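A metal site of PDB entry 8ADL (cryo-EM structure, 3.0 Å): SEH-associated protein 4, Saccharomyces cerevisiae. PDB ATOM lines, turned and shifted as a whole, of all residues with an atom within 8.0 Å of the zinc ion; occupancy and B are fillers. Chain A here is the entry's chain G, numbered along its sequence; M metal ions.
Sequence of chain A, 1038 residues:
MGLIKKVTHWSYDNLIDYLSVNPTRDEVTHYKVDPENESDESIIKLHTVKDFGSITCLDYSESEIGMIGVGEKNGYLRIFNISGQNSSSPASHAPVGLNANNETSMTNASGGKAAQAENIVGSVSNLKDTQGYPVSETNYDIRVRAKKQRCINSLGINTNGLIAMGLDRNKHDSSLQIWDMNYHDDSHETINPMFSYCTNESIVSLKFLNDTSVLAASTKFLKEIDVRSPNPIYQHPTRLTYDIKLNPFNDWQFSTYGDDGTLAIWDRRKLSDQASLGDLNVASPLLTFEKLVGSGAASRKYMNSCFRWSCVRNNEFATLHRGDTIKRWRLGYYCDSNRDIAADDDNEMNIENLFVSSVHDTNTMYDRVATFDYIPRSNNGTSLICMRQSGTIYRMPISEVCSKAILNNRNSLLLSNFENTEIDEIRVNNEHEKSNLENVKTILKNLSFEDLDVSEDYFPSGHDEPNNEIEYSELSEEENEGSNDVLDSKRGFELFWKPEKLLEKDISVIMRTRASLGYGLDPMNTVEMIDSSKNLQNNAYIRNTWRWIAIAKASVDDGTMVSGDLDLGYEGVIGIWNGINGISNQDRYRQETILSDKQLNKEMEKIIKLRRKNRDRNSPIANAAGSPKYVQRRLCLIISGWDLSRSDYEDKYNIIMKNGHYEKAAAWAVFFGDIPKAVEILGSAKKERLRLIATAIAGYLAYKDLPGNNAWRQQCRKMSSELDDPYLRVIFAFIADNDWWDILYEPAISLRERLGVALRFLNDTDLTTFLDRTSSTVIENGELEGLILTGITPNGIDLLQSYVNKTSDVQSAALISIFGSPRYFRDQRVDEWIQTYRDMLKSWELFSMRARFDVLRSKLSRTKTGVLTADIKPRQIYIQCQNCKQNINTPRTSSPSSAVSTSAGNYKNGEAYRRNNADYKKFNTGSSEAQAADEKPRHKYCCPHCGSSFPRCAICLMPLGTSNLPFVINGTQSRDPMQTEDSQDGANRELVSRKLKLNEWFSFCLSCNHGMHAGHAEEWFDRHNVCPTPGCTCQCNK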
ATOM      1  N   GLN A 880     -15.404  10.849 -14.219  1.00  0.00           N
ATOM      2  CA  GLN A 880     -16.380  11.859 -14.583  1.00  0.00           C
ATOM      3  C   GLN A 880     -16.300  12.140 -16.084  1.00  0.00           C
ATOM      4  O   GLN A 880     -15.535  11.525 -16.821  1.00  0.00           O
ATOM      5  CB  GLN A 880     -16.159  13.137 -13.775  1.00  0.00           C
ATOM      6  CG  GLN A 880     -16.452  12.997 -12.291  1.00  0.00           C
ATOM      7  CD  GLN A 880     -16.440  14.328 -11.569  1.00  0.00           C
ATOM      8  OE1 GLN A 880     -15.912  15.314 -12.074  1.00  0.00           O
ATOM      9  NE2 GLN A 880     -17.013  14.360 -10.373  1.00  0.00           N
ATOM     10  N   CYS A 881     -17.114  13.102 -16.545  1.00  0.00           N
ATOM     11  CA  CYS A 881     -17.132  13.488 -17.950  1.00  0.00           C
ATOM     12  C   CYS A 881     -17.102  14.995 -18.167  1.00  0.00           C
ATOM     13  O   CYS A 881     -16.951  15.411 -19.319  1.00  0.00           O
ATOM     14  CB  CYS A 881     -18.364  12.904 -18.664  1.00  0.00           C
ATOM     15  SG  CYS A 881     -19.923  13.746 -18.315  1.00  0.00           S
ATOM     16  N   GLN A 882     -17.301  15.806 -17.122  1.00  0.00           N
ATOM     17  CA  GLN A 882     -17.190  17.263 -17.124  1.00  0.00           C
ATOM     18  C   GLN A 882     -18.235  17.945 -18.024  1.00  0.00           C
ATOM     19  O   GLN A 882     -18.164  19.154 -18.244  1.00  0.00           O
ATOM     20  CB  GLN A 882     -15.773  17.732 -17.507  1.00  0.00           C
ATOM     21  CG  GLN A 882     -15.321  19.023 -16.812  1.00  0.00           C
ATOM     22  CD  GLN A 882     -13.957  19.489 -17.297  1.00  0.00           C
ATOM     23  OE1 GLN A 882     -13.391  18.918 -18.217  1.00  0.00           O
ATOM     24  NE2 GLN A 882     -13.444  20.542 -16.664  1.00  0.00           N
ATOM     25  N   ASN A 883     -19.213  17.197 -18.530  1.00  0.00           N
ATOM     26  CA  ASN A 883     -20.337  17.736 -19.264  1.00  0.00           C
ATOM     27  C   ASN A 883     -21.648  17.628 -18.510  1.00  0.00           C
ATOM     28  O   ASN A 883     -22.497  18.515 -18.612  1.00  0.00           O
ATOM     29  CB  ASN A 883     -20.475  17.037 -20.625  1.00  0.00           C
ATOM     30  CG  ASN A 883     -19.545  17.617 -21.678  1.00  0.00           C
ATOM     31  OD1 ASN A 883     -18.798  16.887 -22.328  1.00  0.00           O
ATOM     32  ND2 ASN A 883     -19.600  18.935 -21.844  1.00  0.00           N
ATOM     33  N   CYS A 884     -21.832  16.554 -17.734  1.00  0.00           N
ATOM     34  CA  CYS A 884     -22.873  16.485 -16.733  1.00  0.00           C
ATOM     35  C   CYS A 884     -22.323  16.210 -15.328  1.00  0.00           C
ATOM     36  O   CYS A 884     -23.105  16.183 -14.379  1.00  0.00           O
ATOM     37  CB  CYS A 884     -23.902  15.416 -17.102  1.00  0.00           C
ATOM     38  SG  CYS A 884     -23.323  13.713 -16.966  1.00  0.00           S
ATOM     39  N   LYS A 885     -21.001  16.019 -15.201  1.00  0.00           N
ATOM     40  CA  LYS A 885     -20.309  15.810 -13.933  1.00  0.00           C
ATOM     41  C   LYS A 885     -20.877  14.623 -13.156  1.00  0.00           C
ATOM     42  O   LYS A 885     -21.165  14.700 -11.960  1.00  0.00           O
ATOM     43  CB  LYS A 885     -20.332  17.075 -13.073  1.00  0.00           C
ATOM     44  CG  LYS A 885     -19.518  18.227 -13.639  1.00  0.00           C
ATOM     45  CD  LYS A 885     -19.684  19.481 -12.806  1.00  0.00           C
ATOM     46  CE  LYS A 885     -18.907  20.651 -13.412  1.00  0.00           C
ATOM     47  NZ  LYS A 885     -19.090  21.902 -12.627  1.00  0.00           N
ATOM     48  N   GLN A 886     -21.031  13.496 -13.852  1.00  0.00           N
ATOM     49  CA  GLN A 886     -21.535  12.264 -13.265  1.00  0.00           C
ATOM     50  C   GLN A 886     -20.630  11.106 -13.655  1.00  0.00           C
ATOM     51  O   GLN A 886     -19.720  11.249 -14.473  1.00  0.00           O
ATOM     52  CB  GLN A 886     -22.979  11.972 -13.718  1.00  0.00           C
ATOM     53  CG  GLN A 886     -24.002  13.001 -13.268  1.00  0.00           C
ATOM     54  CD  GLN A 886     -24.441  12.797 -11.832  1.00  0.00           C
ATOM     55  OE1 GLN A 886     -24.769  11.683 -11.423  1.00  0.00           O
ATOM     56  NE2 GLN A 886     -24.468  13.878 -11.064  1.00  0.00           N
ATOM     57  N   ASN A 887     -20.893   9.955 -13.042  1.00  0.00           N
ATOM     58  CA  ASN A 887     -20.174   8.739 -13.388  1.00  0.00           C
ATOM     59  C   ASN A 887     -20.583   8.267 -14.766  1.00  0.00           C
ATOM     60  O   ASN A 887     -21.755   8.358 -15.151  1.00  0.00           O
ATOM     61  CB  ASN A 887     -20.436   7.658 -12.342  1.00  0.00           C
ATOM     62  CG  ASN A 887     -19.340   6.606 -12.307  1.00  0.00           C
ATOM     63  OD1 ASN A 887     -18.341   6.706 -13.025  1.00  0.00           O
ATOM     64  ND2 ASN A 887     -19.513   5.590 -11.466  1.00  0.00           N
ATOM     65  N   ILE A 888     -19.616   7.753 -15.541  1.00  0.00           N
ATOM     66  CA  ILE A 888     -19.916   7.293 -16.887  1.00  0.00           C
ATOM     67  C   ILE A 888     -20.317   5.822 -16.922  1.00  0.00           C
ATOM     68  O   ILE A 888     -20.660   5.308 -18.001  1.00  0.00           O
ATOM     69  CB  ILE A 888     -18.715   7.500 -17.840  1.00  0.00           C
ATOM     70  CG1 ILE A 888     -17.631   6.464 -17.564  1.00  0.00           C
ATOM     71  CG2 ILE A 888     -18.164   8.907 -17.681  1.00  0.00           C
ATOM     72  CD1 ILE A 888     -16.650   6.314 -18.699  1.00  0.00           C
ATOM     73  N   CYS A 942     -20.646   6.713 -25.606  1.00  0.00           N
ATOM     74  CA  CYS A 942     -21.178   8.019 -25.227  1.00  0.00           C
ATOM     75  C   CYS A 942     -21.493   8.000 -23.739  1.00  0.00           C
ATOM     76  O   CYS A 942     -21.614   6.930 -23.122  1.00  0.00           O
ATOM     77  CB  CYS A 942     -22.432   8.379 -26.027  1.00  0.00           C
ATOM     78  SG  CYS A 942     -22.108   9.072 -27.653  1.00  0.00           S
ATOM     79  N   CYS A 943     -21.601   9.187 -23.156  1.00  0.00           N
ATOM     80  CA  CYS A 943     -21.947   9.274 -21.740  1.00  0.00           C
ATOM     81  C   CYS A 943     -23.409   8.878 -21.541  1.00  0.00           C
ATOM     82  O   CYS A 943     -24.277   9.356 -22.276  1.00  0.00           O
ATOM     83  CB  CYS A 943     -21.714  10.698 -21.219  1.00  0.00           C
ATOM     84  SG  CYS A 943     -22.251  10.957 -19.511  1.00  0.00           S
ATOM     85  N   PRO A 944     -23.711   8.012 -20.576  1.00  0.00           N
ATOM     86  CA  PRO A 944     -25.087   7.552 -20.382  1.00  0.00           C
ATOM     87  C   PRO A 944     -26.001   8.546 -19.662  1.00  0.00           C
ATOM     88  O   PRO A 944     -27.154   8.204 -19.395  1.00  0.00           O
ATOM     89  CB  PRO A 944     -24.916   6.270 -19.534  1.00  0.00           C
ATOM     90  CG  PRO A 944     -23.452   5.957 -19.587  1.00  0.00           C
ATOM     91  CD  PRO A 944     -22.767   7.273 -19.728  1.00  0.00           C
ATOM     92  N   HIS A 945     -25.517   9.746 -19.348  1.00  0.00           N
ATOM     93  CA  HIS A 945     -26.363  10.743 -18.705  1.00  0.00           C
ATOM     94  C   HIS A 945     -26.478  12.066 -19.468  1.00  0.00           C
ATOM     95  O   HIS A 945     -27.434  12.805 -19.225  1.00  0.00           O
ATOM     96  CB  HIS A 945     -25.834  11.057 -17.289  1.00  0.00           C
ATOM     97  CG  HIS A 945     -25.871   9.886 -16.363  1.00  0.00           C
ATOM     98  ND1 HIS A 945     -26.751   8.833 -16.523  1.00  0.00           N
ATOM     99  CD2 HIS A 945     -25.129   9.588 -15.267  1.00  0.00           C
ATOM    100  CE1 HIS A 945     -26.554   7.953 -15.561  1.00  0.00           C
ATOM    101  NE2 HIS A 945     -25.573   8.384 -14.784  1.00  0.00           N
ATOM    102  N   CYS A 946     -25.543  12.368 -20.371  1.00  0.00           N
ATOM    103  CA  CYS A 946     -25.656  13.584 -21.172  1.00  0.00           C
ATOM    104  C   CYS A 946     -25.336  13.369 -22.644  1.00  0.00           C
ATOM    105  O   CYS A 946     -25.464  14.317 -23.419  1.00  0.00           O
ATOM    106  CB  CYS A 946     -24.739  14.683 -20.604  1.00  0.00           C
ATOM    107  SG  CYS A 946     -22.965  14.351 -20.735  1.00  0.00           S
ATOM    108  N   GLY A 947     -24.915  12.169 -23.046  1.00  0.00           N
ATOM    109  CA  GLY A 947     -24.711  11.865 -24.444  1.00  0.00           C
ATOM    110  C   GLY A 947     -23.458  12.466 -25.068  1.00  0.00           C
ATOM    111  O   GLY A 947     -23.288  12.364 -26.278  1.00  0.00           O
ATOM    112  N   SER A 948     -22.607  13.094 -24.270  1.00  0.00           N
ATOM    113  CA  SER A 948     -21.400  13.712 -24.810  1.00  0.00           C
ATOM    114  C   SER A 948     -20.401  12.641 -25.244  1.00  0.00           C
ATOM    115  O   SER A 948     -20.411  11.509 -24.741  1.00  0.00           O
ATOM    116  CB  SER A 948     -20.754  14.633 -23.772  1.00  0.00           C
ATOM    117  OG  SER A 948     -19.634  15.301 -24.311  1.00  0.00           O
ATOM    118  N   SER A 949     -19.548  12.996 -26.192  1.00  0.00           N
ATOM    119  CA  SER A 949     -18.649  12.024 -26.789  1.00  0.00           C
ATOM    120  C   SER A 949     -17.493  11.704 -25.860  1.00  0.00           C
ATOM    121  O   SER A 949     -16.910  12.592 -25.242  1.00  0.00           O
ATOM    122  CB  SER A 949     -18.107  12.554 -28.124  1.00  0.00           C
ATOM    123  OG  SER A 949     -19.141  12.661 -29.090  1.00  0.00           O
ATOM    124  N   PHE A 950     -17.178  10.411 -25.761  1.00  0.00           N
ATOM    125  CA  PHE A 950     -16.054   9.977 -24.965  1.00  0.00           C
ATOM    126  C   PHE A 950     -14.746  10.289 -25.695  1.00  0.00           C
ATOM    127  O   PHE A 950     -14.711  10.334 -26.929  1.00  0.00           O
ATOM    128  CB  PHE A 950     -16.136   8.484 -24.676  1.00  0.00           C
ATOM    129  CG  PHE A 950     -17.066   8.135 -23.555  1.00  0.00           C
ATOM    130  CD1 PHE A 950     -17.491   9.096 -22.648  1.00  0.00           C
ATOM    131  CD2 PHE A 950     -17.528   6.831 -23.402  1.00  0.00           C
ATOM    132  CE1 PHE A 950     -18.344   8.777 -21.616  1.00  0.00           C
ATOM    133  CE2 PHE A 950     -18.384   6.503 -22.366  1.00  0.00           C
ATOM    134  CZ  PHE A 950     -18.789   7.484 -21.476  1.00  0.00           C
HETATM  135 ZN    ZN M   1     -22.112  13.204 -18.884  1.00  0.00          ZN
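The zinc ion is bound by the side-chain sulfur (SG) of Cys 884, the side-chain sulfur (SG) of Cys 881, the side-chain sulfur (SG) of Cys 943 and the side-chain sulfur (SG) of Cys 946.
The backbone NH of Asn 883 lies close to the side-chain sulfur of Cys 881.
N of His 945 sits close to SG of Cys 943 (3.5 Å).
The backbone NH (N) of Cys 943 sits at hydrogen-bond distance from the backbone carbonyl oxygen (O) of Ser 948 (3.1 Å).
The backbone NH (N) of Ser 948 sits close to the side-chain sulfur (SG) of Cys 946 (3.8 Å).
Along chain A the residues within 4 Å of the zinc ion span positions 881 to 946.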
